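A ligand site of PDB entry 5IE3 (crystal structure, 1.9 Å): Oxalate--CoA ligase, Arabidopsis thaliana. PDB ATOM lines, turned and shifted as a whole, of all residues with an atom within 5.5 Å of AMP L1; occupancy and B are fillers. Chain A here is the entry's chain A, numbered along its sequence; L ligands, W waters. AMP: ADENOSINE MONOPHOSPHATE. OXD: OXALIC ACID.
Water W5 lies within hydrogen-bond range of O5' of AMP L1 (2.4 Å), OG of Ser 171 (3.2 Å), NH2 of Arg 409 (3.2 Å) and NZ of Lys 500 (3.5 Å). Water W1 bridges an oxygen (O3P) of AMP L1 (2.5 Å) and an oxygen (O3) of OXD L2 (3.2 Å). Water W2 lies within hydrogen-bond range of N1 of AMP L1 (2.8 Å), OE2 of Glu 310 (3.1 Å) and OG of Ser 291 (3.3 Å). Water W4 lies within hydrogen-bond range of the side-chain hydroxyl (OG) of Ser 171 (2.9 Å) and an oxygen (O2P) of AMP L1 (3.1 Å).
O3P of AMP L1 sits close to O3 of OXD L2 (2.5 Å).
The backbone NH of Ala 313 sits close to the side-chain sulfur of Cys 288 (3.7 Å). The side-chain amino group (NZ) of Lys 500 sits at hydrogen-bond distance from the backbone carbonyl oxygen (O) of Ser 289 (2.9 Å). OD2 of Asp 394 is in hydrogen-bond range of OH of Tyr 312 (2.7 Å). OG1 of Thr 392 lies within hydrogen-bond range of OH of Tyr 312 (3.3 Å). The backbone carbonyl oxygen of Tyr 312 sits at hydrogen-bond distance from the backbone NH of Met 321 (2.8 Å). The side-chain carboxylate (OE2) of Glu 310 is in hydrogen-bond range of the backbone NH (N) of Leu 292 (2.9 Å). The backbone NH (N) of Ala 311 lies within hydrogen-bond range of the backbone carbonyl oxygen (O) of Ser 287 (2.8 Å). N of Asp 394 lies within hydrogen-bond range of OG1 of Thr 392 (3.0 Å).
Residues that only touch AMP L1: Ala 313 (3.2 Å), Ala 290 (3.4 Å), Val 337 (3.4 Å), Met 314 (3.5 Å), Leu 406 (3.7 Å) and Tyr 312 (3.7 Å). Hydrophobic or aromatic side chains within 4 Å of AMP L1: Tyr 312, Met 314, Val 337 and Leu 406. 15 residues have an atom within 4 Å of AMP L1: Ser 171, Ser 289, Ala 290, Ser 291, Glu 310, Ala 311, Tyr 312, Ala 313, Met 314, Thr 315, Val 337, Asp 394, Leu 406, Arg 409 and Lys 500.
A nitrogen (N6) of AMP L1 lies within hydrogen-bond range of the backbone carbonyl oxygen (O) of Ala 311 (2.7 Å). The side-chain hydroxyl (OG) of Ser 289 sits at hydrogen-bond distance from an oxygen (O6) of OXD L2 (2.5 Å). The side-chain hydroxyl of Thr 315 is in hydrogen-bond range of an oxygen (O1P) of AMP L1 (3.1 Å). O4' of AMP L1 is in hydrogen-bond range of NH2 of Arg 409 (3.4 Å). The backbone NH of Thr 315 lies within hydrogen-bond range of an oxygen (O1P) of AMP L1. O3P of AMP L1 is in salt-bridge range of NZ of Lys 500, 3.1 Å away. The side-chain sulfur (SG) of Cys 288 sits at hydrogen-bond distance from an oxygen (O6) of OXD L2 (3.7 Å). The side-chain amino group of Lys 500 lies within salt-bridge range of an oxygen (O5) of OXD L2, at 2.8 Å. An oxygen (O2P) of AMP L1 is in hydrogen-bond range of the side-chain hydroxyl (OG) of Ser 171 (3.1 Å). The backbone NH of Ser 291 sits close to a nitrogen (N1) of AMP L1 (3.3 Å). N7 of AMP L1 sits at hydrogen-bond distance from N of Ser 289, at 3.2 Å. The backbone NH of Met 314 lies within hydrogen-bond range of an oxygen (O4) of OXD L2 (3.4 Å). An oxygen (O2') of AMP L1 sits at hydrogen-bond distance from the side-chain carboxylate (OD1) of Asp 394 (2.5 Å). The side-chain carboxylate of Glu 310 is in hydrogen-bond range of a nitrogen (N6) of AMP L1, at 3.1 Å.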
ATOM      1  N   THR A 170       1.671 -12.559  -5.164  1.00  0.00           N
ATOM      2  CA  THR A 170       0.507 -11.681  -4.968  1.00  0.00           C
ATOM      3  C   THR A 170       0.421 -11.176  -3.519  1.00  0.00           C
ATOM      4  O   THR A 170       1.014 -11.778  -2.602  1.00  0.00           O
ATOM      5  CB  THR A 170      -0.795 -12.395  -5.346  1.00  0.00           C
ATOM      6  OG1 THR A 170      -0.965 -13.560  -4.540  1.00  0.00           O
ATOM      7  CG2 THR A 170      -0.756 -12.777  -6.842  1.00  0.00           C
ATOM      8  N   SER A 171      -0.324 -10.087  -3.334  1.00  0.00           N
ATOM      9  CA  SER A 171      -0.433  -9.326  -2.077  1.00  0.00           C
ATOM     10  C   SER A 171      -1.135  -9.983  -0.905  1.00  0.00           C
ATOM     11  O   SER A 171      -0.849  -9.666   0.249  1.00  0.00           O
ATOM     12  CB  SER A 171      -1.177  -8.022  -2.351  1.00  0.00           C
ATOM     13  OG  SER A 171      -2.521  -8.308  -2.696  1.00  0.00           O
ATOM     14  N   THR A 173      -4.350  -9.589  -0.179  1.00  0.00           N
ATOM     15  CA  THR A 173      -5.342  -8.661   0.380  1.00  0.00           C
ATOM     16  C   THR A 173      -6.678  -9.344   0.652  1.00  0.00           C
ATOM     17  O   THR A 173      -7.253  -9.199   1.726  1.00  0.00           O
ATOM     18  CB  THR A 173      -5.593  -7.431  -0.570  1.00  0.00           C
ATOM     19  OG1 THR A 173      -6.250  -7.867  -1.767  1.00  0.00           O
ATOM     20  CG2 THR A 173      -4.308  -6.702  -0.922  1.00  0.00           C
ATOM     21  N   SER A 287      -1.398   7.807 -12.298  1.00  0.00           N
ATOM     22  CA  SER A 287      -1.740   7.136 -11.032  1.00  0.00           C
ATOM     23  C   SER A 287      -2.182   5.700 -11.333  1.00  0.00           C
ATOM     24  O   SER A 287      -2.804   5.473 -12.374  1.00  0.00           O
ATOM     25  CB  SER A 287      -2.864   7.880 -10.278  1.00  0.00           C
ATOM     26  OG  SER A 287      -3.146   7.256  -9.031  1.00  0.00           O
ATOM     27  N   CYS A 288      -1.873   4.749 -10.459  1.00  0.00           N
ATOM     28  CA  CYS A 288      -2.261   3.340 -10.636  1.00  0.00           C
ATOM     29  C   CYS A 288      -2.151   2.620  -9.298  1.00  0.00           C
ATOM     30  O   CYS A 288      -1.577   3.190  -8.316  1.00  0.00           O
ATOM     31  CB  CYS A 288      -1.361   2.648 -11.703  1.00  0.00           C
ATOM     32  SG  CYS A 288      -2.006   1.046 -12.339  1.00  0.00           S
ATOM     33  N   SER A 289      -2.705   1.406  -9.248  1.00  0.00           N
ATOM     34  CA  SER A 289      -2.583   0.386  -8.152  1.00  0.00           C
ATOM     35  C   SER A 289      -3.674   0.429  -7.063  1.00  0.00           C
ATOM     36  O   SER A 289      -3.882  -0.559  -6.363  1.00  0.00           O
ATOM     37  CB  SER A 289      -1.226   0.450  -7.434  1.00  0.00           C
ATOM     38  OG  SER A 289      -0.133   0.314  -8.336  1.00  0.00           O
ATOM     39  N   ALA A 290      -4.312   1.587  -6.881  1.00  0.00           N
ATOM     40  CA  ALA A 290      -5.431   1.747  -5.933  1.00  0.00           C
ATOM     41  C   ALA A 290      -6.252   2.911  -6.447  1.00  0.00           C
ATOM     42  O   ALA A 290      -5.741   3.720  -7.227  1.00  0.00           O
ATOM     43  CB  ALA A 290      -4.927   2.006  -4.471  1.00  0.00           C
ATOM     44  N   SER A 291      -7.501   3.008  -6.023  1.00  0.00           N
ATOM     45  CA  SER A 291      -8.368   4.019  -6.601  1.00  0.00           C
ATOM     46  C   SER A 291      -7.870   5.449  -6.374  1.00  0.00           C
ATOM     47  O   SER A 291      -7.535   5.805  -5.236  1.00  0.00           O
ATOM     48  CB  SER A 291      -9.764   3.850  -6.045  1.00  0.00           C
ATOM     49  OG  SER A 291     -10.632   4.746  -6.694  1.00  0.00           O
ATOM     50  N   LEU A 292      -7.798   6.228  -7.456  1.00  0.00           N
ATOM     51  CA  LEU A 292      -7.536   7.683  -7.401  1.00  0.00           C
ATOM     52  C   LEU A 292      -8.832   8.442  -7.199  1.00  0.00           C
ATOM     53  O   LEU A 292      -9.634   8.547  -8.133  1.00  0.00           O
ATOM     54  CB  LEU A 292      -6.881   8.185  -8.708  1.00  0.00           C
ATOM     55  CG  LEU A 292      -6.425   9.665  -8.682  1.00  0.00           C
ATOM     56  CD1 LEU A 292      -5.383   9.942  -7.598  1.00  0.00           C
ATOM     57  CD2 LEU A 292      -5.970  10.205 -10.037  1.00  0.00           C
ATOM     58  N   GLU A 310      -5.207   8.114 -14.968  1.00  0.00           N
ATOM     59  CA  GLU A 310      -5.304   6.946 -14.089  1.00  0.00           C
ATOM     60  C   GLU A 310      -5.304   5.641 -14.901  1.00  0.00           C
ATOM     61  O   GLU A 310      -5.962   5.548 -15.949  1.00  0.00           O
ATOM     62  CB  GLU A 310      -6.574   7.014 -13.233  1.00  0.00           C
ATOM     63  CG  GLU A 310      -6.550   5.935 -12.164  1.00  0.00           C
ATOM     64  CD  GLU A 310      -7.725   5.958 -11.215  1.00  0.00           C
ATOM     65  OE1 GLU A 310      -8.711   6.689 -11.474  1.00  0.00           O
ATOM     66  OE2 GLU A 310      -7.650   5.213 -10.208  1.00  0.00           O
ATOM     67  N   ALA A 311      -4.570   4.659 -14.404  1.00  0.00           N
ATOM     68  CA  ALA A 311      -4.531   3.324 -14.992  1.00  0.00           C
ATOM     69  C   ALA A 311      -4.914   2.266 -13.960  1.00  0.00           C
ATOM     70  O   ALA A 311      -4.968   2.535 -12.747  1.00  0.00           O
ATOM     71  CB  ALA A 311      -3.114   3.019 -15.573  1.00  0.00           C
ATOM     72  N   TYR A 312      -5.205   1.072 -14.462  1.00  0.00           N
ATOM     73  CA  TYR A 312      -5.581  -0.113 -13.692  1.00  0.00           C
ATOM     74  C   TYR A 312      -4.612  -1.248 -14.079  1.00  0.00           C
ATOM     75  O   TYR A 312      -4.350  -1.460 -15.275  1.00  0.00           O
ATOM     76  CB  TYR A 312      -7.046  -0.450 -13.994  1.00  0.00           C
ATOM     77  CG  TYR A 312      -7.552  -1.821 -13.635  1.00  0.00           C
ATOM     78  CD1 TYR A 312      -7.507  -2.309 -12.309  1.00  0.00           C
ATOM     79  CD2 TYR A 312      -8.201  -2.595 -14.600  1.00  0.00           C
ATOM     80  CE1 TYR A 312      -8.058  -3.586 -12.000  1.00  0.00           C
ATOM     81  CE2 TYR A 312      -8.744  -3.827 -14.304  1.00  0.00           C
ATOM     82  CZ  TYR A 312      -8.685  -4.313 -13.005  1.00  0.00           C
ATOM     83  OH  TYR A 312      -9.245  -5.556 -12.766  1.00  0.00           O
ATOM     84  N   ALA A 313      -4.086  -1.945 -13.071  1.00  0.00           N
ATOM     85  CA  ALA A 313      -2.988  -2.884 -13.264  1.00  0.00           C
ATOM     86  C   ALA A 313      -2.943  -3.958 -12.159  1.00  0.00           C
ATOM     87  O   ALA A 313      -3.494  -3.765 -11.055  1.00  0.00           O
ATOM     88  CB  ALA A 313      -1.644  -2.125 -13.329  1.00  0.00           C
ATOM     89  N   MET A 314      -2.296  -5.085 -12.459  1.00  0.00           N
ATOM     90  CA  MET A 314      -2.106  -6.097 -11.428  1.00  0.00           C
ATOM     91  C   MET A 314      -0.939  -6.989 -11.807  1.00  0.00           C
ATOM     92  O   MET A 314      -0.508  -7.053 -12.987  1.00  0.00           O
ATOM     93  CB  MET A 314      -3.394  -6.943 -11.216  1.00  0.00           C
ATOM     94  CG  MET A 314      -3.720  -7.930 -12.358  1.00  0.00           C
ATOM     95  SD  MET A 314      -5.462  -8.491 -12.228  1.00  0.00           S
ATOM     96  CE  MET A 314      -5.543  -9.237 -10.585  1.00  0.00           C
ATOM     97  N   THR A 315      -0.442  -7.687 -10.805  1.00  0.00           N
ATOM     98  CA  THR A 315       0.728  -8.525 -10.982  1.00  0.00           C
ATOM     99  C   THR A 315       0.492  -9.552 -12.112  1.00  0.00           C
ATOM    100  O   THR A 315       1.361  -9.730 -12.959  1.00  0.00           O
ATOM    101  CB  THR A 315       1.109  -9.246  -9.667  1.00  0.00           C
ATOM    102  OG1 THR A 315       1.268  -8.266  -8.618  1.00  0.00           O
ATOM    103  CG2 THR A 315       2.407 -10.013  -9.858  1.00  0.00           C
ATOM    104  N   GLU A 316      -0.674 -10.190 -12.121  1.00  0.00           N
ATOM    105  CA  GLU A 316      -0.956 -11.245 -13.107  1.00  0.00           C
ATOM    106  C   GLU A 316      -1.015 -10.748 -14.555  1.00  0.00           C
ATOM    107  O   GLU A 316      -0.914 -11.556 -15.489  1.00  0.00           O
ATOM    108  CB  GLU A 316      -2.276 -11.968 -12.763  1.00  0.00           C
ATOM    109  CG  GLU A 316      -2.200 -12.814 -11.479  1.00  0.00           C
ATOM    110  CD  GLU A 316      -2.666 -12.032 -10.233  1.00  0.00           C
ATOM    111  OE1 GLU A 316      -2.438 -10.806 -10.175  1.00  0.00           O
ATOM    112  OE2 GLU A 316      -3.235 -12.669  -9.318  1.00  0.00           O
ATOM    113  N   MET A 321      -3.386  -3.063 -17.341  1.00  0.00           N
ATOM    114  CA  MET A 321      -4.557  -3.597 -18.029  1.00  0.00           C
ATOM    115  C   MET A 321      -5.271  -2.500 -18.812  1.00  0.00           C
ATOM    116  O   MET A 321      -5.522  -2.640 -20.030  1.00  0.00           O
ATOM    117  CB  MET A 321      -5.499  -4.238 -17.009  1.00  0.00           C
ATOM    118  CG  MET A 321      -4.947  -5.577 -16.489  1.00  0.00           C
ATOM    119  SD  MET A 321      -5.997  -6.326 -15.242  1.00  0.00           S
ATOM    120  CE  MET A 321      -5.615  -5.245 -13.820  1.00  0.00           C
ATOM    121  N   VAL A 337     -10.807   4.115 -14.831  1.00  0.00           N
ATOM    122  CA  VAL A 337      -9.453   3.673 -15.153  1.00  0.00           C
ATOM    123  C   VAL A 337      -9.267   3.462 -16.665  1.00  0.00           C
ATOM    124  O   VAL A 337      -8.323   2.772 -17.123  1.00  0.00           O
ATOM    125  CB  VAL A 337      -9.066   2.376 -14.364  1.00  0.00           C
ATOM    126  CG1 VAL A 337      -8.996   2.671 -12.874  1.00  0.00           C
ATOM    127  CG2 VAL A 337     -10.058   1.253 -14.602  1.00  0.00           C
ATOM    128  N   THR A 392     -10.008 -11.365 -12.803  1.00  0.00           N
ATOM    129  CA  THR A 392      -9.217 -10.455 -11.964  1.00  0.00           C
ATOM    130  C   THR A 392      -9.631 -10.427 -10.493  1.00  0.00           C
ATOM    131  O   THR A 392      -8.845  -9.992  -9.661  1.00  0.00           O
ATOM    132  CB  THR A 392      -9.281  -8.985 -12.431  1.00  0.00           C
ATOM    133  OG1 THR A 392     -10.637  -8.519 -12.327  1.00  0.00           O
ATOM    134  CG2 THR A 392      -8.791  -8.862 -13.880  1.00  0.00           C
ATOM    135  N   ASP A 394     -11.912  -8.402  -9.612  1.00  0.00           N
ATOM    136  CA  ASP A 394     -12.452  -7.036  -9.492  1.00  0.00           C
ATOM    137  C   ASP A 394     -13.805  -6.934 -10.157  1.00  0.00           C
ATOM    138  O   ASP A 394     -14.015  -7.466 -11.244  1.00  0.00           O
ATOM    139  CB  ASP A 394     -11.505  -6.007 -10.125  1.00  0.00           C
ATOM    140  CG  ASP A 394     -10.169  -5.942  -9.429  1.00  0.00           C
ATOM    141  OD1 ASP A 394     -10.122  -5.800  -8.163  1.00  0.00           O
ATOM    142  OD2 ASP A 394      -9.130  -6.081 -10.144  1.00  0.00           O
ATOM    143  N   LEU A 406     -14.237   0.951 -11.844  1.00  0.00           N
ATOM    144  CA  LEU A 406     -14.096  -0.109 -10.857  1.00  0.00           C
ATOM    145  C   LEU A 406     -15.000   0.133  -9.667  1.00  0.00           C
ATOM    146  O   LEU A 406     -15.126   1.266  -9.171  1.00  0.00           O
ATOM    147  CB  LEU A 406     -12.644  -0.218 -10.402  1.00  0.00           C
ATOM    148  CG  LEU A 406     -11.699  -0.669 -11.533  1.00  0.00           C
ATOM    149  CD1 LEU A 406     -10.252  -0.518 -11.054  1.00  0.00           C
ATOM    150  CD2 LEU A 406     -12.001  -2.088 -11.973  1.00  0.00           C
ATOM    151  N   ARG A 409     -12.889  -4.872  -5.198  1.00  0.00           N
ATOM    152  CA  ARG A 409     -12.630  -6.316  -5.115  1.00  0.00           C
ATOM    153  C   ARG A 409     -13.900  -7.024  -4.672  1.00  0.00           C
ATOM    154  O   ARG A 409     -14.581  -6.536  -3.769  1.00  0.00           O
ATOM    155  CB  ARG A 409     -11.483  -6.629  -4.149  1.00  0.00           C
ATOM    156  CG  ARG A 409     -10.150  -5.998  -4.577  1.00  0.00           C
ATOM    157  CD  ARG A 409      -9.023  -6.306  -3.588  1.00  0.00           C
ATOM    158  NE  ARG A 409      -7.723  -5.715  -3.969  1.00  0.00           N
ATOM    159  CZ  ARG A 409      -7.369  -4.458  -3.701  1.00  0.00           C
ATOM    160  NH1 ARG A 409      -8.221  -3.635  -3.087  1.00  0.00           N
ATOM    161  NH2 ARG A 409      -6.173  -4.007  -4.085  1.00  0.00           N
ATOM    162  N   ILE A 424     -14.628   1.889  -2.427  1.00  0.00           N
ATOM    163  CA  ILE A 424     -13.982   2.876  -3.321  1.00  0.00           C
ATOM    164  C   ILE A 424     -14.782   4.208  -3.359  1.00  0.00           C
ATOM    165  O   ILE A 424     -14.219   5.317  -3.163  1.00  0.00           O
ATOM    166  CB  ILE A 424     -13.839   2.281  -4.771  1.00  0.00           C
ATOM    167  CG1 ILE A 424     -12.675   1.283  -4.808  1.00  0.00           C
ATOM    168  CG2 ILE A 424     -13.601   3.378  -5.833  1.00  0.00           C
ATOM    169  CD1 ILE A 424     -12.444   0.615  -6.183  1.00  0.00           C
ATOM    170  N   SER A 498       3.693  -1.789  -1.431  1.00  0.00           N
ATOM    171  CA  SER A 498       3.110  -1.315  -2.688  1.00  0.00           C
ATOM    172  C   SER A 498       2.238  -0.032  -2.508  1.00  0.00           C
ATOM    173  O   SER A 498       1.559   0.384  -3.445  1.00  0.00           O
ATOM    174  CB  SER A 498       2.319  -2.430  -3.366  1.00  0.00           C
ATOM    175  OG  SER A 498       1.477  -3.094  -2.453  1.00  0.00           O
ATOM    176  N   LYS A 500      -0.470   0.577  -0.576  1.00  0.00           N
ATOM    177  CA  LYS A 500      -1.912   0.367  -0.405  1.00  0.00           C
ATOM    178  C   LYS A 500      -2.275   0.212   1.064  1.00  0.00           C
ATOM    179  O   LYS A 500      -1.530  -0.373   1.848  1.00  0.00           O
ATOM    180  CB  LYS A 500      -2.393  -0.870  -1.176  1.00  0.00           C
ATOM    181  CG  LYS A 500      -1.942  -0.897  -2.627  1.00  0.00           C
ATOM    182  CD  LYS A 500      -2.557  -2.081  -3.421  1.00  0.00           C
ATOM    183  CE  LYS A 500      -1.732  -2.333  -4.701  1.00  0.00           C
ATOM    184  NZ  LYS A 500      -2.518  -3.093  -5.739  1.00  0.00           N
HETATM  185  P   AMP L   1      -1.611  -6.384  -6.797  1.00  0.00           P
HETATM  186  O1P AMP L   1      -1.569  -7.166  -8.093  1.00  0.00           O
HETATM  187  O2P AMP L   1      -1.795  -7.230  -5.554  1.00  0.00           O
HETATM  188  O3P AMP L   1      -0.549  -5.329  -6.642  1.00  0.00           O
HETATM  189  O5' AMP L   1      -3.008  -5.591  -6.807  1.00  0.00           O
HETATM  190  C5' AMP L   1      -3.847  -5.563  -7.953  1.00  0.00           C
HETATM  191  C4' AMP L   1      -5.218  -5.019  -7.585  1.00  0.00           C
HETATM  192  O4' AMP L   1      -5.132  -3.590  -7.297  1.00  0.00           O
HETATM  193  C3' AMP L   1      -6.256  -5.068  -8.676  1.00  0.00           C
HETATM  194  O3' AMP L   1      -6.785  -6.382  -8.863  1.00  0.00           O
HETATM  195  C2' AMP L   1      -7.285  -4.050  -8.197  1.00  0.00           C
HETATM  196  O2' AMP L   1      -8.096  -4.628  -7.178  1.00  0.00           O
HETATM  197  C1' AMP L   1      -6.378  -2.998  -7.554  1.00  0.00           C
HETATM  198  N9  AMP L   1      -6.136  -1.844  -8.447  1.00  0.00           N
HETATM  199  C8  AMP L   1      -5.130  -1.681  -9.321  1.00  0.00           C
HETATM  200  N7  AMP L   1      -5.229  -0.483  -9.961  1.00  0.00           N
HETATM  201  C5  AMP L   1      -6.332   0.138  -9.449  1.00  0.00           C
HETATM  202  C6  AMP L   1      -7.037   1.423  -9.646  1.00  0.00           C
HETATM  203  N6  AMP L   1      -6.548   2.325 -10.532  1.00  0.00           N
HETATM  204  N1  AMP L   1      -8.155   1.651  -8.919  1.00  0.00           N
HETATM  205  C2  AMP L   1      -8.625   0.756  -8.021  1.00  0.00           C
HETATM  206  N3  AMP L   1      -8.039  -0.429  -7.799  1.00  0.00           N
HETATM  207  C4  AMP L   1      -6.915  -0.768  -8.465  1.00  0.00           C
HETATM  208  C1  OXD L   2      -0.404  -3.373  -8.983  1.00  0.00           C
HETATM  209  C2  OXD L   2      -0.032  -2.627 -10.202  1.00  0.00           C
HETATM  210  O3  OXD L   2      -0.011  -4.581  -8.938  1.00  0.00           O
HETATM  211  O4  OXD L   2       0.306  -3.404 -11.140  1.00  0.00           O
HETATM  212  O5  OXD L   2      -1.066  -2.768  -8.115  1.00  0.00           O
HETATM  213  O6  OXD L   2      -0.057  -1.353 -10.255  1.00  0.00           O
HETATM  214  O   HOH W   1       1.783  -4.589  -6.302  1.00  0.00           O
HETATM  215  O   HOH W   2     -10.180   3.432  -9.721  1.00  0.00           O
HETATM  216  O   HOH W   3      -9.594  -2.153  -6.267  1.00  0.00           O
HETATM  217  O   HOH W   4      -3.281  -9.899  -4.941  1.00  0.00           O
HETATM  218  O   HOH W   5      -3.813  -6.105  -4.552  1.00  0.00           O
HETATM  219  O   HOH W   6      -6.065  -8.420  -7.155  1.00  0.00           O
